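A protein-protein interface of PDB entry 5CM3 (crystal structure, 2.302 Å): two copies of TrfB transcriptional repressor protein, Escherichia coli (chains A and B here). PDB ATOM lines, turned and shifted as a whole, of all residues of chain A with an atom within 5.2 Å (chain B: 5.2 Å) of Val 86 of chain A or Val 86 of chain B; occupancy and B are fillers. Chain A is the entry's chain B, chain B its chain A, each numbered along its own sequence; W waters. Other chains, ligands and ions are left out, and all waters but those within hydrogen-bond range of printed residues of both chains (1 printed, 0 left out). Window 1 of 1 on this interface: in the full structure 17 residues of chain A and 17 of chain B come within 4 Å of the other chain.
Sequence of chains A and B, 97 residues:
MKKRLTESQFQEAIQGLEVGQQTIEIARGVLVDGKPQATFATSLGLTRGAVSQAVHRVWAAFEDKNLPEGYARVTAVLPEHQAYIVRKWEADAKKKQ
N of Val 74 of chain B lies within hydrogen-bond range of O of Ala 76 of chain A (2.8 Å). NE2 of Gln 82 of chain A sits close to NE1 of Trp 89 of chain B, at 3.2 Å. The backbone carbonyl oxygen (O) of Ala 76 of chain B sits at hydrogen-bond distance from the backbone NH (N) of Val 74 of chain A, 3.0 Å away.
Among the printed residues, merely in contact across the chains: Ala 76 of chain A with Glu 90 of chain B (3.1 Å), Glu 90 of chain A with Ala 76 of chain B (3.2 Å), Trp 89 of chain A with Gln 82 of chain B (3.4 Å), Ala 76 of chain A with Val 86 of chain B (3.6 Å), Glu 90 of chain A with Leu 78 of chain B (3.8 Å), Val 86 of chain A with Trp 89 of chain B (3.9 Å), Val 74 of chain A with Val 74 of chain B (3.9 Å), Trp 89 of chain A with Leu 78 of chain B (3.9 Å), Ile 85 of chain A with Trp 89 of chain B (3.9 Å), Val 74 of chain A with Arg 87 of chain B (3.9 Å), Leu 78 of chain A with Trp 89 of chain B (3.9 Å), Val 86 of chain A with Val 86 of chain B (3.96 Å) and Trp 89 of chain A with Ile 85 of chain B (3.99 Å).
Of chain B, only Val 86 and Trp 89 come within 4 Å of Val 86 of chain A. Val 86 of chain B touches just these residues of chain A: Ala 76 and Val 86. Printed residues of chain A within 4 Å of Ala 76 of chain B: Val 74 and Glu 90. Of the printed residues of chain A, Leu 78 of chain B touches Trp 89 and Glu 90. Of the printed residues of chain B, Val 74 of chain A touches Val 74 (3.9 Å), Ala 76 (3.0 Å) and Arg 87 (3.9 Å). Lys 88 of chain A touches none of the printed residues of chain B. The nearest residue of chain B that does not touch Val 86 of chain A is Val 74 of chain B (4.1 Å). The nearest residue of chain A that does not touch Val 86 of chain B is Leu 78 of chain A (4.2 Å). The nearest printed residue of chain B that does not touch Trp 89 of chain A is Trp 89 of chain B (4.2 Å).
Hydrophobic or aromatic side chains of chain A within 4 Å of the printed part of chain B: Val 74, Ala 76, Leu 78, Ile 85, Val 86 and Trp 89. Along chain A the printed residues that touch a printed residue of chain B span positions 74 to 90. Of the 13 printed residues of chain B, 9 touch a printed residue of chain A. Among the printed residues, 16 pairs touch across the chains. Among the printed residues, no Asp or Glu carboxylate lies within 4 Å of a Lys or Arg side-chain nitrogen of the other chain.
Val 74 of chain A touches Ala 76 of chain B, and with the chains exchanged Ala 76 of chain A touches Val 74 of chain B. Val 74 of chain A touches Arg 87 of chain B, but with the chains exchanged Arg 87 of chain A does not touch Val 74 of chain B (4.3 Å). Ala 76 of chain A touches Val 86 of chain B, but with the chains exchanged Val 86 of chain A does not touch Ala 76 of chain B (4.3 Å). Glu 90 of chain A touches Leu 78 of chain B, but with the chains exchanged Leu 78 of chain A does not touch Glu 90 of chain B (4.6 Å). Of the 16 pairs that touch across the chains among the printed residues, 12 have their exchanged pair printed and touching as well.
Water W1 bridges the backbone carbonyl oxygen (O) of Trp 89 of chain A (2.5 Å) and the side-chain amide oxygen (OE1) of Gln 82 of chain B (2.5 Å).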
ATOM      1  N   VAL A  74     -30.428 -20.416 -14.013  1.00  0.00           N
ATOM      2  CA  VAL A  74     -29.180 -21.157 -13.979  1.00  0.00           C
ATOM      3  C   VAL A  74     -28.866 -21.606 -12.572  1.00  0.00           C
ATOM      4  O   VAL A  74     -29.239 -20.952 -11.592  1.00  0.00           O
ATOM      5  CB  VAL A  74     -28.014 -20.339 -14.568  1.00  0.00           C
ATOM      6  CG1 VAL A  74     -27.676 -19.198 -13.648  1.00  0.00           C
ATOM      7  CG2 VAL A  74     -26.793 -21.238 -14.811  1.00  0.00           C
ATOM      8  N   ALA A  76     -25.714 -23.451 -10.071  1.00  0.00           N
ATOM      9  CA  ALA A  76     -24.321 -23.811  -9.964  1.00  0.00           C
ATOM     10  C   ALA A  76     -23.823 -23.837  -8.537  1.00  0.00           C
ATOM     11  O   ALA A  76     -24.389 -23.212  -7.623  1.00  0.00           O
ATOM     12  CB  ALA A  76     -23.482 -22.861 -10.794  1.00  0.00           C
ATOM     13  N   LEU A  78     -20.543 -22.808  -6.630  1.00  0.00           N
ATOM     14  CA  LEU A  78     -19.466 -21.861  -6.795  1.00  0.00           C
ATOM     15  C   LEU A  78     -18.838 -21.551  -5.432  1.00  0.00           C
ATOM     16  O   LEU A  78     -19.433 -21.847  -4.388  1.00  0.00           O
ATOM     17  CB  LEU A  78     -20.025 -20.574  -7.375  1.00  0.00           C
ATOM     18  CG  LEU A  78     -20.738 -20.682  -8.716  1.00  0.00           C
ATOM     19  CD1 LEU A  78     -21.474 -19.393  -9.041  1.00  0.00           C
ATOM     20  CD2 LEU A  78     -19.742 -21.017  -9.826  1.00  0.00           C
ATOM     21  N   GLN A  82     -18.145 -15.852  -5.511  1.00  0.00           N
ATOM     22  CA  GLN A  82     -18.811 -15.852  -6.785  1.00  0.00           C
ATOM     23  C   GLN A  82     -20.277 -16.010  -6.573  1.00  0.00           C
ATOM     24  O   GLN A  82     -21.061 -15.459  -7.345  1.00  0.00           O
ATOM     25  CB  GLN A  82     -18.271 -16.942  -7.703  1.00  0.00           C
ATOM     26  CG  GLN A  82     -16.914 -16.540  -8.307  1.00  0.00           C
ATOM     27  CD  GLN A  82     -16.288 -17.610  -9.188  1.00  0.00           C
ATOM     28  OE1 GLN A  82     -16.693 -18.784  -9.169  1.00  0.00           O
ATOM     29  NE2 GLN A  82     -15.287 -17.222  -9.961  1.00  0.00           N
ATOM     30  N   ALA A  83     -20.672 -16.743  -5.544  1.00  0.00           N
ATOM     31  CA  ALA A  83     -22.095 -16.888  -5.262  1.00  0.00           C
ATOM     32  C   ALA A  83     -22.628 -15.525  -4.809  1.00  0.00           C
ATOM     33  O   ALA A  83     -23.709 -15.099  -5.208  1.00  0.00           O
ATOM     34  CB  ALA A  83     -22.348 -17.957  -4.208  1.00  0.00           C
ATOM     35  N   TYR A  84     -21.848 -14.833  -4.000  1.00  0.00           N
ATOM     36  CA  TYR A  84     -22.182 -13.474  -3.598  1.00  0.00           C
ATOM     37  C   TYR A  84     -22.465 -12.620  -4.828  1.00  0.00           C
ATOM     38  O   TYR A  84     -23.465 -11.906  -4.885  1.00  0.00           O
ATOM     39  CB  TYR A  84     -21.053 -12.866  -2.747  1.00  0.00           C
ATOM     40  CG  TYR A  84     -21.125 -11.359  -2.552  1.00  0.00           C
ATOM     41  CD1 TYR A  84     -22.182 -10.753  -1.865  1.00  0.00           C
ATOM     42  CD2 TYR A  84     -20.104 -10.534  -3.028  1.00  0.00           C
ATOM     43  CE1 TYR A  84     -22.216  -9.367  -1.686  1.00  0.00           C
ATOM     44  CE2 TYR A  84     -20.141  -9.165  -2.853  1.00  0.00           C
ATOM     45  CZ  TYR A  84     -21.183  -8.585  -2.187  1.00  0.00           C
ATOM     46  OH  TYR A  84     -21.179  -7.210  -2.038  1.00  0.00           O
ATOM     47  N   ILE A  85     -21.595 -12.722  -5.826  1.00  0.00           N
ATOM     48  CA  ILE A  85     -21.751 -11.968  -7.064  1.00  0.00           C
ATOM     49  C   ILE A  85     -23.043 -12.339  -7.796  1.00  0.00           C
ATOM     50  O   ILE A  85     -23.724 -11.478  -8.370  1.00  0.00           O
ATOM     51  CB  ILE A  85     -20.535 -12.199  -8.008  1.00  0.00           C
ATOM     52  CG1 ILE A  85     -19.339 -11.398  -7.495  1.00  0.00           C
ATOM     53  CG2 ILE A  85     -20.859 -11.774  -9.439  1.00  0.00           C
ATOM     54  CD1 ILE A  85     -17.993 -11.752  -8.135  1.00  0.00           C
ATOM     55  N   VAL A  86     -23.381 -13.618  -7.806  1.00  0.00           N
ATOM     56  CA  VAL A  86     -24.579 -14.021  -8.512  1.00  0.00           C
ATOM     57  C   VAL A  86     -25.799 -13.489  -7.762  1.00  0.00           C
ATOM     58  O   VAL A  86     -26.698 -12.945  -8.384  1.00  0.00           O
ATOM     59  CB  VAL A  86     -24.625 -15.515  -8.687  1.00  0.00           C
ATOM     60  CG1 VAL A  86     -26.014 -15.970  -9.231  1.00  0.00           C
ATOM     61  CG2 VAL A  86     -23.501 -15.929  -9.613  1.00  0.00           C
ATOM     62  N   ARG A  87     -25.822 -13.596  -6.434  1.00  0.00           N
ATOM     63  CA  ARG A  87     -26.939 -13.068  -5.652  1.00  0.00           C
ATOM     64  C   ARG A  87     -27.127 -11.567  -5.826  1.00  0.00           C
ATOM     65  O   ARG A  87     -28.248 -11.066  -5.843  1.00  0.00           O
ATOM     66  CB  ARG A  87     -26.707 -13.316  -4.173  1.00  0.00           C
ATOM     67  CG  ARG A  87     -26.742 -14.744  -3.739  1.00  0.00           C
ATOM     68  CD  ARG A  87     -26.370 -14.804  -2.255  1.00  0.00           C
ATOM     69  NE  ARG A  87     -25.892 -16.124  -1.879  1.00  0.00           N
ATOM     70  CZ  ARG A  87     -24.726 -16.390  -1.296  1.00  0.00           C
ATOM     71  NH1 ARG A  87     -23.829 -15.426  -0.962  1.00  0.00           N
ATOM     72  NH2 ARG A  87     -24.457 -17.662  -1.034  1.00  0.00           N
ATOM     73  N   LYS A  88     -26.014 -10.853  -5.902  1.00  0.00           N
ATOM     74  CA  LYS A  88     -26.016  -9.414  -6.108  1.00  0.00           C
ATOM     75  C   LYS A  88     -26.673  -9.122  -7.476  1.00  0.00           C
ATOM     76  O   LYS A  88     -27.616  -8.328  -7.576  1.00  0.00           O
ATOM     77  CB  LYS A  88     -24.562  -8.904  -6.001  1.00  0.00           C
ATOM     78  CG  LYS A  88     -24.318  -7.434  -6.337  1.00  0.00           C
ATOM     79  CD  LYS A  88     -24.799  -6.470  -5.243  1.00  0.00           C
ATOM     80  CE  LYS A  88     -25.178  -5.067  -5.815  1.00  0.00           C
ATOM     81  NZ  LYS A  88     -26.485  -5.069  -6.570  1.00  0.00           N
ATOM     82  N   TRP A  89     -26.190  -9.797  -8.514  1.00  0.00           N
ATOM     83  CA  TRP A  89     -26.719  -9.657  -9.872  1.00  0.00           C
ATOM     84  C   TRP A  89     -28.218  -9.950  -9.920  1.00  0.00           C
ATOM     85  O   TRP A  89     -29.006  -9.189 -10.503  1.00  0.00           O
ATOM     86  CB  TRP A  89     -26.024 -10.668 -10.814  1.00  0.00           C
ATOM     87  CG  TRP A  89     -24.707 -10.248 -11.303  1.00  0.00           C
ATOM     88  CD1 TRP A  89     -24.178  -8.984 -11.242  1.00  0.00           C
ATOM     89  CD2 TRP A  89     -23.724 -11.060 -11.948  1.00  0.00           C
ATOM     90  NE1 TRP A  89     -22.937  -8.967 -11.814  1.00  0.00           N
ATOM     91  CE2 TRP A  89     -22.633 -10.230 -12.259  1.00  0.00           C
ATOM     92  CE3 TRP A  89     -23.653 -12.396 -12.295  1.00  0.00           C
ATOM     93  CZ2 TRP A  89     -21.489 -10.699 -12.886  1.00  0.00           C
ATOM     94  CZ3 TRP A  89     -22.510 -12.863 -12.922  1.00  0.00           C
ATOM     95  CH2 TRP A  89     -21.461 -12.026 -13.212  1.00  0.00           C
ATOM     96  N   GLU A  90     -28.586 -11.085  -9.332  1.00  0.00           N
ATOM     97  CA  GLU A  90     -29.947 -11.589  -9.355  1.00  0.00           C
ATOM     98  C   GLU A  90     -30.909 -10.677  -8.615  1.00  0.00           C
ATOM     99  O   GLU A  90     -32.107 -10.664  -8.912  1.00  0.00           O
ATOM    100  CB  GLU A  90     -29.996 -12.958  -8.703  1.00  0.00           C
ATOM    101  CG  GLU A  90     -31.122 -13.098  -7.694  1.00  0.00           C
ATOM    102  CD  GLU A  90     -31.203 -14.496  -7.098  1.00  0.00           C
ATOM    103  OE1 GLU A  90     -30.200 -14.972  -6.501  1.00  0.00           O
ATOM    104  OE2 GLU A  90     -32.275 -15.122  -7.228  1.00  0.00           O
ATOM    105  N   ALA A  91     -30.390  -9.927  -7.648  1.00  0.00           N
ATOM    106  CA  ALA A  91     -31.213  -8.993  -6.890  1.00  0.00           C
ATOM    107  C   ALA A  91     -31.611  -7.812  -7.783  1.00  0.00           C
ATOM    108  O   ALA A  91     -32.697  -7.226  -7.637  1.00  0.00           O
ATOM    109  CB  ALA A  91     -30.470  -8.513  -5.670  1.00  0.00           C
ATOM    110  N   VAL B  74     -26.037 -21.950  -5.785  1.00  0.00           N
ATOM    111  CA  VAL B  74     -26.881 -20.818  -6.063  1.00  0.00           C
ATOM    112  C   VAL B  74     -27.780 -20.988  -7.314  1.00  0.00           C
ATOM    113  O   VAL B  74     -27.399 -21.656  -8.272  1.00  0.00           O
ATOM    114  CB  VAL B  74     -26.030 -19.553  -6.131  1.00  0.00           C
ATOM    115  CG1 VAL B  74     -25.146 -19.541  -7.374  1.00  0.00           C
ATOM    116  CG2 VAL B  74     -26.907 -18.323  -6.032  1.00  0.00           C
ATOM    117  N   ALA B  76     -30.649 -18.631  -9.766  1.00  0.00           N
ATOM    118  CA  ALA B  76     -31.243 -17.352 -10.059  1.00  0.00           C
ATOM    119  C   ALA B  76     -31.544 -17.234 -11.537  1.00  0.00           C
ATOM    120  O   ALA B  76     -30.917 -17.909 -12.361  1.00  0.00           O
ATOM    121  CB  ALA B  76     -30.291 -16.246  -9.637  1.00  0.00           C
ATOM    122  N   LEU B  78     -30.977 -15.009 -14.600  1.00  0.00           N
ATOM    123  CA  LEU B  78     -30.014 -13.984 -14.961  1.00  0.00           C
ATOM    124  C   LEU B  78     -30.098 -13.614 -16.423  1.00  0.00           C
ATOM    125  O   LEU B  78     -30.494 -14.438 -17.267  1.00  0.00           O
ATOM    126  CB  LEU B  78     -28.586 -14.461 -14.681  1.00  0.00           C
ATOM    127  CG  LEU B  78     -28.151 -14.661 -13.229  1.00  0.00           C
ATOM    128  CD1 LEU B  78     -26.716 -15.178 -13.211  1.00  0.00           C
ATOM    129  CD2 LEU B  78     -28.306 -13.396 -12.398  1.00  0.00           C
ATOM    130  N   GLN B  82     -24.498 -12.536 -17.937  1.00  0.00           N
ATOM    131  CA  GLN B  82     -24.274 -12.969 -16.546  1.00  0.00           C
ATOM    132  C   GLN B  82     -24.476 -14.482 -16.414  1.00  0.00           C
ATOM    133  O   GLN B  82     -23.725 -15.166 -15.715  1.00  0.00           O
ATOM    134  CB  GLN B  82     -25.223 -12.219 -15.593  1.00  0.00           C
ATOM    135  CG  GLN B  82     -24.745 -10.784 -15.267  1.00  0.00           C
ATOM    136  CD  GLN B  82     -25.769  -9.919 -14.532  1.00  0.00           C
ATOM    137  OE1 GLN B  82     -26.860 -10.379 -14.146  1.00  0.00           O
ATOM    138  NE2 GLN B  82     -25.424  -8.637 -14.362  1.00  0.00           N
ATOM    139  N   ALA B  83     -25.473 -15.009 -17.119  1.00  0.00           N
ATOM    140  CA  ALA B  83     -25.698 -16.458 -17.166  1.00  0.00           C
ATOM    141  C   ALA B  83     -24.547 -17.199 -17.861  1.00  0.00           C
ATOM    142  O   ALA B  83     -24.068 -18.230 -17.377  1.00  0.00           O
ATOM    143  CB  ALA B  83     -26.996 -16.755 -17.852  1.00  0.00           C
ATOM    144  N   TYR B  84     -24.100 -16.661 -18.985  1.00  0.00           N
ATOM    145  CA  TYR B  84     -22.952 -17.195 -19.700  1.00  0.00           C
ATOM    146  C   TYR B  84     -21.741 -17.308 -18.765  1.00  0.00           C
ATOM    147  O   TYR B  84     -20.982 -18.276 -18.816  1.00  0.00           O
ATOM    148  CB  TYR B  84     -22.634 -16.265 -20.880  1.00  0.00           C
ATOM    149  CG  TYR B  84     -21.435 -16.668 -21.703  1.00  0.00           C
ATOM    150  CD1 TYR B  84     -20.146 -16.599 -21.181  1.00  0.00           C
ATOM    151  CD2 TYR B  84     -21.588 -17.091 -23.009  1.00  0.00           C
ATOM    152  CE1 TYR B  84     -19.054 -16.962 -21.920  1.00  0.00           C
ATOM    153  CE2 TYR B  84     -20.494 -17.449 -23.766  1.00  0.00           C
ATOM    154  CZ  TYR B  84     -19.222 -17.384 -23.211  1.00  0.00           C
ATOM    155  OH  TYR B  84     -18.115 -17.740 -23.957  1.00  0.00           O
ATOM    156  N   ILE B  85     -21.558 -16.302 -17.919  1.00  0.00           N
ATOM    157  CA  ILE B  85     -20.394 -16.250 -17.028  1.00  0.00           C
ATOM    158  C   ILE B  85     -20.448 -17.376 -16.008  1.00  0.00           C
ATOM    159  O   ILE B  85     -19.448 -18.039 -15.735  1.00  0.00           O
ATOM    160  CB  ILE B  85     -20.276 -14.855 -16.328  1.00  0.00           C
ATOM    161  CG1 ILE B  85     -19.838 -13.823 -17.355  1.00  0.00           C
ATOM    162  CG2 ILE B  85     -19.301 -14.887 -15.113  1.00  0.00           C
ATOM    163  CD1 ILE B  85     -20.181 -12.400 -16.969  1.00  0.00           C
ATOM    164  N   VAL B  86     -21.629 -17.620 -15.462  1.00  0.00           N
ATOM    165  CA  VAL B  86     -21.784 -18.736 -14.548  1.00  0.00           C
ATOM    166  C   VAL B  86     -21.440 -20.033 -15.268  1.00  0.00           C
ATOM    167  O   VAL B  86     -20.715 -20.853 -14.726  1.00  0.00           O
ATOM    168  CB  VAL B  86     -23.181 -18.794 -13.907  1.00  0.00           C
ATOM    169  CG1 VAL B  86     -23.216 -19.875 -12.864  1.00  0.00           C
ATOM    170  CG2 VAL B  86     -23.509 -17.466 -13.266  1.00  0.00           C
ATOM    171  N   ARG B  87     -21.922 -20.196 -16.494  1.00  0.00           N
ATOM    172  CA  ARG B  87     -21.626 -21.400 -17.270  1.00  0.00           C
ATOM    173  C   ARG B  87     -20.126 -21.567 -17.424  1.00  0.00           C
ATOM    174  O   ARG B  87     -19.585 -22.656 -17.220  1.00  0.00           O
ATOM    175  CB  ARG B  87     -22.223 -21.312 -18.672  1.00  0.00           C
ATOM    176  CG  ARG B  87     -23.739 -21.247 -18.738  1.00  0.00           C
ATOM    177  CD  ARG B  87     -24.314 -22.546 -18.273  1.00  0.00           C
ATOM    178  NE  ARG B  87     -25.773 -22.647 -18.396  1.00  0.00           N
ATOM    179  CZ  ARG B  87     -26.492 -23.670 -17.893  1.00  0.00           C
ATOM    180  NH1 ARG B  87     -25.882 -24.653 -17.208  1.00  0.00           N
ATOM    181  NH2 ARG B  87     -27.820 -23.711 -18.051  1.00  0.00           N
ATOM    182  N   LYS B  88     -19.467 -20.472 -17.794  1.00  0.00           N
ATOM    183  CA  LYS B  88     -18.031 -20.474 -17.998  1.00  0.00           C
ATOM    184  C   LYS B  88     -17.290 -20.746 -16.676  1.00  0.00           C
ATOM    185  O   LYS B  88     -16.327 -21.506 -16.670  1.00  0.00           O
ATOM    186  CB  LYS B  88     -17.591 -19.163 -18.661  1.00  0.00           C
ATOM    187  CG  LYS B  88     -16.083 -18.895 -18.680  1.00  0.00           C
ATOM    188  CD  LYS B  88     -15.290 -19.868 -19.548  1.00  0.00           C
ATOM    189  CE  LYS B  88     -15.566 -19.695 -21.023  1.00  0.00           C
ATOM    190  NZ  LYS B  88     -15.405 -18.295 -21.467  1.00  0.00           N
ATOM    191  N   TRP B  89     -17.753 -20.170 -15.563  1.00  0.00           N
ATOM    192  CA  TRP B  89     -17.125 -20.417 -14.255  1.00  0.00           C
ATOM    193  C   TRP B  89     -17.070 -21.923 -13.946  1.00  0.00           C
ATOM    194  O   TRP B  89     -16.001 -22.479 -13.651  1.00  0.00           O
ATOM    195  CB  TRP B  89     -17.896 -19.696 -13.132  1.00  0.00           C
ATOM    196  CG  TRP B  89     -17.477 -18.248 -12.897  1.00  0.00           C
ATOM    197  CD1 TRP B  89     -16.304 -17.652 -13.282  1.00  0.00           C
ATOM    198  CD2 TRP B  89     -18.246 -17.223 -12.254  1.00  0.00           C
ATOM    199  NE1 TRP B  89     -16.294 -16.335 -12.915  1.00  0.00           N
ATOM    200  CE2 TRP B  89     -17.469 -16.040 -12.280  1.00  0.00           C
ATOM    201  CE3 TRP B  89     -19.507 -17.187 -11.654  1.00  0.00           C
ATOM    202  CZ2 TRP B  89     -17.915 -14.830 -11.731  1.00  0.00           C
ATOM    203  CZ3 TRP B  89     -19.947 -15.981 -11.107  1.00  0.00           C
ATOM    204  CH2 TRP B  89     -19.149 -14.826 -11.152  1.00  0.00           C
ATOM    205  N   GLU B  90     -18.240 -22.559 -14.017  1.00  0.00           N
ATOM    206  CA  GLU B  90     -18.409 -24.009 -13.861  1.00  0.00           C
ATOM    207  C   GLU B  90     -17.545 -24.802 -14.836  1.00  0.00           C
ATOM    208  O   GLU B  90     -16.678 -25.585 -14.422  1.00  0.00           O
ATOM    209  CB  GLU B  90     -19.868 -24.362 -14.142  1.00  0.00           C
ATOM    210  CG  GLU B  90     -20.795 -24.186 -12.969  1.00  0.00           C
ATOM    211  CD  GLU B  90     -22.253 -24.491 -13.312  1.00  0.00           C
ATOM    212  OE1 GLU B  90     -22.798 -23.930 -14.299  1.00  0.00           O
ATOM    213  OE2 GLU B  90     -22.860 -25.308 -12.583  1.00  0.00           O
ATOM    214  N   ALA B  91     -17.817 -24.592 -16.130  1.00  0.00           N
ATOM    215  CA  ALA B  91     -17.150 -25.293 -17.229  1.00  0.00           C
ATOM    216  C   ALA B  91     -15.629 -25.159 -17.190  1.00  0.00           C
ATOM    217  O   ALA B  91     -14.925 -26.054 -17.649  1.00  0.00           O
ATOM    218  CB  ALA B  91     -17.696 -24.806 -18.590  1.00  0.00           C
HETATM  219  O   HOH W   1     -28.595  -8.916 -12.990  1.00  0.00           O
